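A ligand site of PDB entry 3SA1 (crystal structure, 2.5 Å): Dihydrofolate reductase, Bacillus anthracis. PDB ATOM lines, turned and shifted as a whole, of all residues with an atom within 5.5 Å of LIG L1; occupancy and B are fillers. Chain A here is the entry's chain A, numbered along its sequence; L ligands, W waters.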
ATOM      1  N   MET A   9     -23.085  -3.815  11.018  1.00  0.00           N
ATOM      2  CA  MET A   9     -22.466  -4.218   9.757  1.00  0.00           C
ATOM      3  C   MET A   9     -21.442  -5.281  10.078  1.00  0.00           C
ATOM      4  O   MET A   9     -20.470  -5.026  10.802  1.00  0.00           O
ATOM      5  CB  MET A   9     -21.814  -3.018   9.053  1.00  0.00           C
ATOM      6  CG  MET A   9     -20.950  -3.378   7.844  1.00  0.00           C
ATOM      7  SD  MET A   9     -21.831  -4.103   6.434  1.00  0.00           S
ATOM      8  CE  MET A   9     -22.855  -2.745   5.869  1.00  0.00           C
ATOM      9  N   VAL A  10     -21.658  -6.479   9.551  1.00  0.00           N
ATOM     10  CA  VAL A  10     -20.881  -7.644   9.966  1.00  0.00           C
ATOM     11  C   VAL A  10     -20.832  -8.738   8.892  1.00  0.00           C
ATOM     12  O   VAL A  10     -21.788  -8.919   8.134  1.00  0.00           O
ATOM     13  CB  VAL A  10     -21.410  -8.224  11.297  1.00  0.00           C
ATOM     14  CG1 VAL A  10     -22.788  -8.882  11.113  1.00  0.00           C
ATOM     15  CG2 VAL A  10     -20.412  -9.222  11.893  1.00  0.00           C
ATOM     16  N   ALA A  11     -19.696  -9.425   8.819  1.00  0.00           N
ATOM     17  CA  ALA A  11     -19.564 -10.640   8.039  1.00  0.00           C
ATOM     18  C   ALA A  11     -19.191 -11.777   8.992  1.00  0.00           C
ATOM     19  O   ALA A  11     -18.285 -11.637   9.792  1.00  0.00           O
ATOM     20  CB  ALA A  11     -18.507 -10.464   6.962  1.00  0.00           C
ATOM     21  N   ASN A  23      -7.571 -10.530  13.527  1.00  0.00           N
ATOM     22  CA  ASN A  23      -7.645 -10.236  12.098  1.00  0.00           C
ATOM     23  C   ASN A  23      -8.846 -10.973  11.499  1.00  0.00           C
ATOM     24  O   ASN A  23      -9.529 -11.734  12.192  1.00  0.00           O
ATOM     25  CB  ASN A  23      -6.352 -10.694  11.412  1.00  0.00           C
ATOM     26  CG  ASN A  23      -5.923  -9.785  10.232  1.00  0.00           C
ATOM     27  OD1 ASN A  23      -6.748  -9.194   9.521  1.00  0.00           O
ATOM     28  ND2 ASN A  23      -4.603  -9.705  10.020  1.00  0.00           N
ATOM     29  N   LEU A  24      -9.092 -10.743  10.208  1.00  0.00           N
ATOM     30  CA  LEU A  24     -10.109 -11.437   9.431  1.00  0.00           C
ATOM     31  C   LEU A  24      -9.640 -12.803   8.953  1.00  0.00           C
ATOM     32  O   LEU A  24      -8.511 -12.933   8.488  1.00  0.00           O
ATOM     33  CB  LEU A  24     -10.505 -10.592   8.213  1.00  0.00           C
ATOM     34  CG  LEU A  24     -11.200  -9.259   8.487  1.00  0.00           C
ATOM     35  CD1 LEU A  24     -11.225  -8.471   7.195  1.00  0.00           C
ATOM     36  CD2 LEU A  24     -12.629  -9.446   9.061  1.00  0.00           C
ATOM     37  N   TRP A  26     -10.660 -14.500   6.368  1.00  0.00           N
ATOM     38  CA  TRP A  26     -10.844 -14.683   4.927  1.00  0.00           C
ATOM     39  C   TRP A  26     -10.494 -13.394   4.169  1.00  0.00           C
ATOM     40  O   TRP A  26     -10.461 -12.314   4.743  1.00  0.00           O
ATOM     41  CB  TRP A  26     -12.296 -15.074   4.632  1.00  0.00           C
ATOM     42  CG  TRP A  26     -13.273 -14.124   5.279  1.00  0.00           C
ATOM     43  CD1 TRP A  26     -13.628 -12.876   4.824  1.00  0.00           C
ATOM     44  CD2 TRP A  26     -13.984 -14.322   6.499  1.00  0.00           C
ATOM     45  NE1 TRP A  26     -14.521 -12.293   5.685  1.00  0.00           N
ATOM     46  CE2 TRP A  26     -14.762 -13.164   6.724  1.00  0.00           C
ATOM     47  CE3 TRP A  26     -14.048 -15.367   7.440  1.00  0.00           C
ATOM     48  CZ2 TRP A  26     -15.592 -13.017   7.855  1.00  0.00           C
ATOM     49  CZ3 TRP A  26     -14.885 -15.219   8.563  1.00  0.00           C
ATOM     50  CH2 TRP A  26     -15.630 -14.054   8.758  1.00  0.00           C
ATOM     51  N   GLU A  31     -16.849  -8.486  -1.089  1.00  0.00           N
ATOM     52  CA  GLU A  31     -17.611  -8.239   0.126  1.00  0.00           C
ATOM     53  C   GLU A  31     -17.196  -6.912   0.754  1.00  0.00           C
ATOM     54  O   GLU A  31     -18.019  -6.189   1.319  1.00  0.00           O
ATOM     55  CB  GLU A  31     -17.411  -9.383   1.114  1.00  0.00           C
ATOM     56  CG  GLU A  31     -18.605  -9.628   2.052  1.00  0.00           C
ATOM     57  CD  GLU A  31     -18.610  -8.739   3.298  1.00  0.00           C
ATOM     58  OE1 GLU A  31     -17.517  -8.359   3.785  1.00  0.00           O
ATOM     59  OE2 GLU A  31     -19.708  -8.412   3.793  1.00  0.00           O
ATOM     60  N   LEU A  32     -15.908  -6.586   0.635  1.00  0.00           N
ATOM     61  CA  LEU A  32     -15.393  -5.318   1.152  1.00  0.00           C
ATOM     62  C   LEU A  32     -15.948  -4.142   0.371  1.00  0.00           C
ATOM     63  O   LEU A  32     -16.191  -3.079   0.939  1.00  0.00           O
ATOM     64  CB  LEU A  32     -13.869  -5.322   1.099  1.00  0.00           C
ATOM     65  CG  LEU A  32     -13.103  -4.203   1.780  1.00  0.00           C
ATOM     66  CD1 LEU A  32     -11.832  -4.772   2.383  1.00  0.00           C
ATOM     67  CD2 LEU A  32     -12.763  -3.159   0.748  1.00  0.00           C
ATOM     68  N   TYR A  34     -18.929  -4.095  -1.174  1.00  0.00           N
ATOM     69  CA  TYR A  34     -20.279  -3.961  -0.683  1.00  0.00           C
ATOM     70  C   TYR A  34     -20.350  -3.139   0.617  1.00  0.00           C
ATOM     71  O   TYR A  34     -21.229  -2.282   0.757  1.00  0.00           O
ATOM     72  CB  TYR A  34     -20.904  -5.347  -0.470  1.00  0.00           C
ATOM     73  CG  TYR A  34     -22.215  -5.334   0.300  1.00  0.00           C
ATOM     74  CD1 TYR A  34     -23.434  -5.170  -0.361  1.00  0.00           C
ATOM     75  CD2 TYR A  34     -22.229  -5.505   1.686  1.00  0.00           C
ATOM     76  CE1 TYR A  34     -24.643  -5.174   0.355  1.00  0.00           C
ATOM     77  CE2 TYR A  34     -23.425  -5.513   2.403  1.00  0.00           C
ATOM     78  CZ  TYR A  34     -24.614  -5.347   1.742  1.00  0.00           C
ATOM     79  OH  TYR A  34     -25.787  -5.352   2.451  1.00  0.00           O
ATOM     80  N   VAL A  35     -19.429  -3.393   1.543  1.00  0.00           N
ATOM     81  CA  VAL A  35     -19.269  -2.628   2.776  1.00  0.00           C
ATOM     82  C   VAL A  35     -19.018  -1.141   2.521  1.00  0.00           C
ATOM     83  O   VAL A  35     -19.630  -0.302   3.189  1.00  0.00           O
ATOM     84  CB  VAL A  35     -18.149  -3.231   3.663  1.00  0.00           C
ATOM     85  CG1 VAL A  35     -17.898  -2.378   4.888  1.00  0.00           C
ATOM     86  CG2 VAL A  35     -18.487  -4.654   4.086  1.00  0.00           C
ATOM     87  N   LYS A  36     -18.134  -0.797   1.578  1.00  0.00           N
ATOM     88  CA  LYS A  36     -17.912   0.618   1.220  1.00  0.00           C
ATOM     89  C   LYS A  36     -19.178   1.269   0.675  1.00  0.00           C
ATOM     90  O   LYS A  36     -19.563   2.351   1.117  1.00  0.00           O
ATOM     91  CB  LYS A  36     -16.760   0.782   0.232  1.00  0.00           C
ATOM     92  CG  LYS A  36     -15.407   0.281   0.752  1.00  0.00           C
ATOM     93  CD  LYS A  36     -14.275   0.644  -0.214  1.00  0.00           C
ATOM     94  CE  LYS A  36     -12.930   0.013   0.207  1.00  0.00           C
ATOM     95  NZ  LYS A  36     -12.171   0.785   1.256  1.00  0.00           N
ATOM     96  N   ASN A  50     -10.622  -3.655  16.910  1.00  0.00           N
ATOM     97  CA  ASN A  50     -11.030  -3.574  15.522  1.00  0.00           C
ATOM     98  C   ASN A  50     -10.349  -2.401  14.829  1.00  0.00           C
ATOM     99  O   ASN A  50      -9.749  -2.597  13.770  1.00  0.00           O
ATOM    100  CB  ASN A  50     -12.552  -3.445  15.381  1.00  0.00           C
ATOM    101  CG  ASN A  50     -13.008  -3.339  13.931  1.00  0.00           C
ATOM    102  OD1 ASN A  50     -12.321  -3.797  13.025  1.00  0.00           O
ATOM    103  ND2 ASN A  50     -14.166  -2.739  13.704  1.00  0.00           N
ATOM    104  N   ALA A  53      -6.588  -2.913  14.156  1.00  0.00           N
ATOM    105  CA  ALA A  53      -6.391  -3.917  13.118  1.00  0.00           C
ATOM    106  C   ALA A  53      -6.645  -3.310  11.734  1.00  0.00           C
ATOM    107  O   ALA A  53      -5.958  -3.651  10.772  1.00  0.00           O
ATOM    108  CB  ALA A  53      -7.282  -5.116  13.362  1.00  0.00           C
ATOM    109  N   ILE A  54      -7.624  -2.413  11.630  1.00  0.00           N
ATOM    110  CA  ILE A  54      -7.833  -1.665  10.408  1.00  0.00           C
ATOM    111  C   ILE A  54      -6.593  -0.802  10.139  1.00  0.00           C
ATOM    112  O   ILE A  54      -5.986  -0.896   9.069  1.00  0.00           O
ATOM    113  CB  ILE A  54      -9.129  -0.820  10.454  1.00  0.00           C
ATOM    114  CG1 ILE A  54     -10.346  -1.736  10.574  1.00  0.00           C
ATOM    115  CG2 ILE A  54      -9.224   0.073   9.222  1.00  0.00           C
ATOM    116  CD1 ILE A  54     -11.633  -1.036  10.774  1.00  0.00           C
ATOM    117  N   ARG A  56      -5.950   2.568  10.150  1.00  0.00           N
ATOM    118  CA  ARG A  56      -6.023   3.898   9.540  1.00  0.00           C
ATOM    119  C   ARG A  56      -7.478   4.398   9.522  1.00  0.00           C
ATOM    120  O   ARG A  56      -8.412   3.591   9.460  1.00  0.00           O
ATOM    121  CB  ARG A  56      -5.463   3.881   8.097  1.00  0.00           C
ATOM    122  CG  ARG A  56      -6.489   3.415   7.036  1.00  0.00           C
ATOM    123  CD  ARG A  56      -5.863   2.799   5.777  1.00  0.00           C
ATOM    124  NE  ARG A  56      -6.895   2.265   4.864  1.00  0.00           N
ATOM    125  CZ  ARG A  56      -7.237   0.983   4.746  1.00  0.00           C
ATOM    126  NH1 ARG A  56      -6.644   0.040   5.473  1.00  0.00           N
ATOM    127  NH2 ARG A  56      -8.177   0.633   3.888  1.00  0.00           N
ATOM    128  N   LEU A  58     -10.846   5.535   7.973  1.00  0.00           N
ATOM    129  CA  LEU A  58     -11.497   5.243   6.705  1.00  0.00           C
ATOM    130  C   LEU A  58     -12.120   6.496   6.075  1.00  0.00           C
ATOM    131  O   LEU A  58     -12.935   7.155   6.709  1.00  0.00           O
ATOM    132  CB  LEU A  58     -12.533   4.112   6.857  1.00  0.00           C
ATOM    133  CG  LEU A  58     -11.988   2.767   7.373  1.00  0.00           C
ATOM    134  CD1 LEU A  58     -13.085   1.737   7.399  1.00  0.00           C
ATOM    135  CD2 LEU A  58     -10.819   2.256   6.537  1.00  0.00           C
ATOM    136  N   ARG A  61     -16.087   9.041   5.958  1.00  0.00           N
ATOM    137  CA  ARG A  61     -16.919   8.574   7.073  1.00  0.00           C
ATOM    138  C   ARG A  61     -16.352   9.131   8.387  1.00  0.00           C
ATOM    139  O   ARG A  61     -15.135   9.278   8.522  1.00  0.00           O
ATOM    140  CB  ARG A  61     -16.947   7.032   7.131  1.00  0.00           C
ATOM    141  CG  ARG A  61     -17.969   6.348   6.222  1.00  0.00           C
ATOM    142  CD  ARG A  61     -17.510   4.947   5.764  1.00  0.00           C
ATOM    143  NE  ARG A  61     -16.217   5.052   5.103  1.00  0.00           N
ATOM    144  CZ  ARG A  61     -15.638   4.107   4.373  1.00  0.00           C
ATOM    145  NH1 ARG A  61     -16.232   2.936   4.169  1.00  0.00           N
ATOM    146  NH2 ARG A  61     -14.458   4.328   3.827  1.00  0.00           N
ATOM    147  N   PHE A  99     -19.632  -1.462  13.701  1.00  0.00           N
ATOM    148  CA  PHE A  99     -18.730  -2.035  12.724  1.00  0.00           C
ATOM    149  C   PHE A  99     -17.828  -3.106  13.346  1.00  0.00           C
ATOM    150  O   PHE A  99     -17.005  -3.693  12.657  1.00  0.00           O
ATOM    151  CB  PHE A  99     -17.889  -0.903  12.125  1.00  0.00           C
ATOM    152  CG  PHE A  99     -17.256  -1.218  10.792  1.00  0.00           C
ATOM    153  CD1 PHE A  99     -18.042  -1.519   9.676  1.00  0.00           C
ATOM    154  CD2 PHE A  99     -15.867  -1.170  10.636  1.00  0.00           C
ATOM    155  CE1 PHE A  99     -17.458  -1.803   8.445  1.00  0.00           C
ATOM    156  CE2 PHE A  99     -15.268  -1.459   9.392  1.00  0.00           C
ATOM    157  CZ  PHE A  99     -16.067  -1.774   8.299  1.00  0.00           C
ATOM    158  N   GLY A 100     -17.994  -3.364  14.645  1.00  0.00           N
ATOM    159  CA  GLY A 100     -17.274  -4.447  15.325  1.00  0.00           C
ATOM    160  C   GLY A 100     -16.117  -3.998  16.196  1.00  0.00           C
ATOM    161  O   GLY A 100     -15.819  -2.805  16.279  1.00  0.00           O
ATOM    162  N   TYR A 105     -20.117  -5.166  19.353  1.00  0.00           N
ATOM    163  CA  TYR A 105     -21.443  -5.704  18.970  1.00  0.00           C
ATOM    164  C   TYR A 105     -22.270  -6.023  20.217  1.00  0.00           C
ATOM    165  O   TYR A 105     -23.435  -5.659  20.261  1.00  0.00           O
ATOM    166  CB  TYR A 105     -21.384  -6.941  18.065  1.00  0.00           C
ATOM    167  CG  TYR A 105     -20.824  -6.736  16.684  1.00  0.00           C
ATOM    168  CD1 TYR A 105     -21.327  -5.758  15.823  1.00  0.00           C
ATOM    169  CD2 TYR A 105     -19.796  -7.543  16.221  1.00  0.00           C
ATOM    170  CE1 TYR A 105     -20.793  -5.570  14.546  1.00  0.00           C
ATOM    171  CE2 TYR A 105     -19.263  -7.385  14.957  1.00  0.00           C
ATOM    172  CZ  TYR A 105     -19.756  -6.393  14.129  1.00  0.00           C
ATOM    173  OH  TYR A 105     -19.208  -6.259  12.875  1.00  0.00           O
ATOM    174  N   TYR A 116     -27.119  -5.573   8.802  1.00  0.00           N
ATOM    175  CA  TYR A 116     -26.496  -5.887   7.518  1.00  0.00           C
ATOM    176  C   TYR A 116     -25.479  -6.992   7.760  1.00  0.00           C
ATOM    177  O   TYR A 116     -24.352  -6.735   8.205  1.00  0.00           O
ATOM    178  CB  TYR A 116     -25.787  -4.675   6.913  1.00  0.00           C
ATOM    179  CG  TYR A 116     -26.652  -3.490   6.594  1.00  0.00           C
ATOM    180  CD1 TYR A 116     -27.027  -2.580   7.582  1.00  0.00           C
ATOM    181  CD2 TYR A 116     -27.082  -3.260   5.295  1.00  0.00           C
ATOM    182  CE1 TYR A 116     -27.830  -1.481   7.293  1.00  0.00           C
ATOM    183  CE2 TYR A 116     -27.888  -2.173   4.994  1.00  0.00           C
ATOM    184  CZ  TYR A 116     -28.255  -1.287   5.986  1.00  0.00           C
ATOM    185  OH  TYR A 116     -29.030  -0.198   5.685  1.00  0.00           O
ATOM    186  N   THR A 118     -23.491 -10.343   6.244  1.00  0.00           N
ATOM    187  CA  THR A 118     -23.013 -11.238   5.203  1.00  0.00           C
ATOM    188  C   THR A 118     -22.734 -12.593   5.827  1.00  0.00           C
ATOM    189  O   THR A 118     -21.993 -12.692   6.811  1.00  0.00           O
ATOM    190  CB  THR A 118     -21.745 -10.692   4.552  1.00  0.00           C
ATOM    191  OG1 THR A 118     -22.039  -9.401   4.018  1.00  0.00           O
ATOM    192  CG2 THR A 118     -21.265 -11.621   3.438  1.00  0.00           C
HETATM  193  N1  LIG L   1     -18.709  -6.038   8.026  1.00  0.00           N
HETATM  194  C1  LIG L   1     -18.704  -6.798   6.916  1.00  0.00           C
HETATM  195  N2  LIG L   1     -17.546  -7.230   6.396  1.00  0.00           N
HETATM  196  C2  LIG L   1     -16.354  -6.931   6.949  1.00  0.00           C
HETATM  197  C3  LIG L   1     -16.340  -6.146   8.112  1.00  0.00           C
HETATM  198  C4  LIG L   1     -17.560  -5.693   8.649  1.00  0.00           C
HETATM  199  C5  LIG L   1     -14.548  -6.547   5.202  1.00  0.00           C
HETATM  200  C6  LIG L   1      -8.392  -5.882   9.532  1.00  0.00           C
HETATM  201  N3  LIG L   1     -19.824  -7.139   6.306  1.00  0.00           N
HETATM  202  N4  LIG L   1     -17.594  -4.937   9.746  1.00  0.00           N
HETATM  203  C7  LIG L   1     -13.989  -5.561   9.205  1.00  0.00           C
HETATM  204  C8  LIG L   1     -15.093  -5.823   8.712  1.00  0.00           C
HETATM  205  C9  LIG L   1     -11.582  -0.415   4.237  1.00  0.00           C
HETATM  206  C10 LIG L   1     -13.750  -0.856   4.922  1.00  0.00           C
HETATM  207  C11 LIG L   1     -11.074  -1.370   5.124  1.00  0.00           C
HETATM  208  C12 LIG L   1     -13.307  -1.831   5.825  1.00  0.00           C
HETATM  209  C13 LIG L   1     -10.109  -3.474   6.721  1.00  0.00           C
HETATM  210  C14 LIG L   1      -9.584  -4.428   7.579  1.00  0.00           C
HETATM  211  C15 LIG L   1     -12.240  -3.673   7.830  1.00  0.00           C
HETATM  212  C16 LIG L   1     -15.117  -7.512   6.247  1.00  0.00           C
HETATM  213  C17 LIG L   1     -12.670  -5.252   9.779  1.00  0.00           C
HETATM  214  N5  LIG L   1     -12.884  -0.169   4.164  1.00  0.00           N
HETATM  215  O1  LIG L   1      -9.827  -5.966   9.400  1.00  0.00           O
HETATM  216  C18 LIG L   1     -11.940  -2.098   5.946  1.00  0.00           C
HETATM  217  C19 LIG L   1     -11.447  -3.081   6.830  1.00  0.00           C
HETATM  218  C20 LIG L   1     -11.724  -4.653   8.707  1.00  0.00           C
HETATM  219  C21 LIG L   1     -10.375  -5.010   8.577  1.00  0.00           C
HETATM  220  P1  LG2 L   2     -13.300  -4.933  19.672  1.00  0.00           P
HETATM  221  O1  LG2 L   2     -14.698  -5.138  20.135  1.00  0.00           O
HETATM  222  O2  LG2 L   2     -13.216  -4.377  18.314  1.00  0.00           O
HETATM  223  O3  LG2 L   2     -12.524  -4.002  20.694  1.00  0.00           O
HETATM  224  C1  LG2 L   2     -12.391  -4.389  22.047  1.00  0.00           C
HETATM  225  C2  LG2 L   2     -12.106  -3.109  22.803  1.00  0.00           C
HETATM  226  O4  LG2 L   2     -13.262  -2.304  22.785  1.00  0.00           O
HETATM  227  C3  LG2 L   2     -11.722  -3.234  24.263  1.00  0.00           C
HETATM  228  O5  LG2 L   2     -10.363  -3.525  24.417  1.00  0.00           O
HETATM  229  C4  LG2 L   2     -12.003  -1.828  24.736  1.00  0.00           C
HETATM  230  O6  LG2 L   2     -10.946  -0.981  24.375  1.00  0.00           O
HETATM  231  C5  LG2 L   2     -13.243  -1.454  23.909  1.00  0.00           C
HETATM  232  N1  LG2 L   2     -14.450  -1.695  24.723  1.00  0.00           N
HETATM  233  C6  LG2 L   2     -15.068  -2.895  24.933  1.00  0.00           C
HETATM  234  N2  LG2 L   2     -16.130  -2.692  25.751  1.00  0.00           N
HETATM  235  C7  LG2 L   2     -16.169  -1.373  26.061  1.00  0.00           C
HETATM  236  C8  LG2 L   2     -17.029  -0.632  26.853  1.00  0.00           C
HETATM  237  N3  LG2 L   2     -18.036  -1.253  27.448  1.00  0.00           N
HETATM  238  N4  LG2 L   2     -16.834   0.728  26.993  1.00  0.00           N
HETATM  239  C9  LG2 L   2     -15.794   1.353  26.354  1.00  0.00           C
HETATM  240  N5  LG2 L   2     -14.938   0.603  25.564  1.00  0.00           N
HETATM  241  C10 LG2 L   2     -15.126  -0.738  25.421  1.00  0.00           C
HETATM  242  O7  LG2 L   2     -12.461  -6.294  19.849  1.00  0.00           O
HETATM  243  P2  LG2 L   2     -12.897  -7.837  19.710  1.00  0.00           P
HETATM  244  O8  LG2 L   2     -11.702  -8.651  20.046  1.00  0.00           O
HETATM  245  O9  LG2 L   2     -14.176  -8.005  20.462  1.00  0.00           O
HETATM  246  O10 LG2 L   2     -13.148  -7.973  18.117  1.00  0.00           O
HETATM  247  C11 LG2 L   2     -12.026  -7.809  17.265  1.00  0.00           C
HETATM  248  C12 LG2 L   2     -11.907  -8.951  16.272  1.00  0.00           C
HETATM  249  O11 LG2 L   2     -13.041  -9.026  15.401  1.00  0.00           O
HETATM  250  C13 LG2 L   2     -10.715  -8.733  15.360  1.00  0.00           C
HETATM  251  O12 LG2 L   2     -10.227 -10.011  14.996  1.00  0.00           O
HETATM  252  C14 LG2 L   2     -11.331  -8.100  14.134  1.00  0.00           C
HETATM  253  O13 LG2 L   2     -10.515  -8.275  13.001  1.00  0.00           O
HETATM  254  C15 LG2 L   2     -12.654  -8.829  14.057  1.00  0.00           C
HETATM  255  N6  LG2 L   2     -13.724  -8.114  13.351  1.00  0.00           N
HETATM  256  C16 LG2 L   2     -14.408  -8.760  12.367  1.00  0.00           C
HETATM  257  C17 LG2 L   2     -15.439  -8.137  11.685  1.00  0.00           C
HETATM  258  C18 LG2 L   2     -16.248  -8.917  10.694  1.00  0.00           C
HETATM  259  O14 LG2 L   2     -17.494  -8.409  10.267  1.00  0.00           O
HETATM  260  N7  LG2 L   2     -15.761 -10.082  10.246  1.00  0.00           N
HETATM  261  C19 LG2 L   2     -15.798  -6.828  12.016  1.00  0.00           C
HETATM  262  C20 LG2 L   2     -15.105  -6.171  13.020  1.00  0.00           C
HETATM  263  C21 LG2 L   2     -14.062  -6.832  13.687  1.00  0.00           C
HETATM  264  P3  LG2 L   2      -9.690  -0.613  25.311  1.00  0.00           P
HETATM  265  O15 LG2 L   2      -8.867  -1.824  25.598  1.00  0.00           O
HETATM  266  O16 LG2 L   2      -8.844   0.373  24.544  1.00  0.00           O
HETATM  267  O17 LG2 L   2     -10.167  -0.078  26.657  1.00  0.00           O
HETATM  268  O   HOH W   1     -10.620  -5.581  12.112  1.00  0.00           O
HETATM  269  O   HOH W   2     -15.204  -9.995   4.092  1.00  0.00           O
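A nitrogen (N3) of LIG L1 is in hydrogen-bond range of the side-chain carboxylate (OE2) of Glu 31, 2.8 Å away.
A nitrogen (N4) of LIG L1 lies within hydrogen-bond range of the backbone carbonyl oxygen (O) of Met 9 (3.1 Å).
A nitrogen (N3) of LIG L1 is in hydrogen-bond range of the side-chain sulfur (SD) of Met 9.
NZ of Lys 36 lies within hydrogen-bond range of N5 of LIG L1.
A nitrogen (N1) of LIG L1 sits close to the backbone NH (N) of Val 10.
The backbone carbonyl oxygen of Val 10 sits close to a nitrogen (N3) of LIG L1 (3.2 Å).
N4 of LIG L1 sits at hydrogen-bond distance from O of Phe 99 (3.2 Å).
An oxygen (O14) of LG2 L2 is in hydrogen-bond range of the backbone NH (N) of Ala 11 (2.8 Å).
The backbone carbonyl oxygen (O) of Ala 11 lies within hydrogen-bond range of a nitrogen (N7) of LG2 L2 (3.0 Å).
The backbone NH of Asn 50 lies within hydrogen-bond range of an oxygen (O2) of LG2 L2, 3.0 Å away.
N of Asn 23 lies within hydrogen-bond range of O12 of LG2 L2, at 3.1 Å.
The backbone carbonyl oxygen of Asn 23 is in hydrogen-bond range of an oxygen (O12) of LG2 L2, at 3.4 Å.
The side-chain carboxylate (OE2) of Glu 31 is in hydrogen-bond range of the side-chain hydroxyl (OG1) of Thr 118, at 2.5 Å.
The backbone carbonyl oxygen of Met 9 sits at hydrogen-bond distance from the side-chain hydroxyl of Tyr 105.
N of Thr 118 lies within hydrogen-bond range of O of Val 10 (2.9 Å).
The backbone carbonyl oxygen (O) of Tyr 116 sits at hydrogen-bond distance from the backbone NH (N) of Val 10, 3.0 Å away.
The backbone carbonyl oxygen (O) of Phe 99 sits at hydrogen-bond distance from the side-chain amide nitrogen (ND2) of Asn 50 (3.2 Å).
The backbone carbonyl oxygen of Phe 99 is in hydrogen-bond range of the side-chain hydroxyl of Tyr 105 (3.4 Å).
The side-chain amide nitrogen (ND2) of Asn 50 lies within hydrogen-bond range of the backbone carbonyl oxygen (O) of Gly 100.
The backbone NH (N) of Ala 11 sits close to a nitrogen (N3) of LIG L1.
Asn 23 touches LIG L1 (OD1 to C6, 3.7 Å).
Leu 24 touches LIG L1 (CD1 to O1, 3.6 Å).
Val 35 touches LIG L1.
Asn 50 touches LIG L1.
Ala 53 touches LIG L1 (O to C6, 3.5 Å).
CG1 of Ile 54 touches C20 of LIG L1, at 3.7 Å.
NH2 of Arg 56 touches C9 of LIG L1 (3.6 Å).
Leu 58 touches LIG L1 (CD2 to C9, 3.6 Å).
OH of Tyr 105 touches N4 of LIG L1 (3.8 Å).
Thr 118 touches LIG L1 (OG1 to N3, 3.9 Å).
Hydrophobic or aromatic side chains within 4 Å of LIG L1: Met 9, Ala 11, Leu 24, Val 35, Ile 54, Leu 58 and Phe 99.
16 residues have an atom within 4 Å of LIG L1: Met 9, Val 10, Ala 11, Asn 23, Leu 24, Glu 31, Val 35, Lys 36, Asn 50, Ala 53, Ile 54, Arg 56, Leu 58, Phe 99, Tyr 105 and Thr 118.
Water W1 lies within hydrogen-bond range of OD1 of Asn 50 (2.6 Å), O13 of LG2 L2 (2.8 Å) and O1 of LIG L1 (2.9 Å).
Water W2 lies within hydrogen-bond range of OE1 of Glu 31 (2.8 Å) and NE1 of Trp 26 (2.9 Å).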
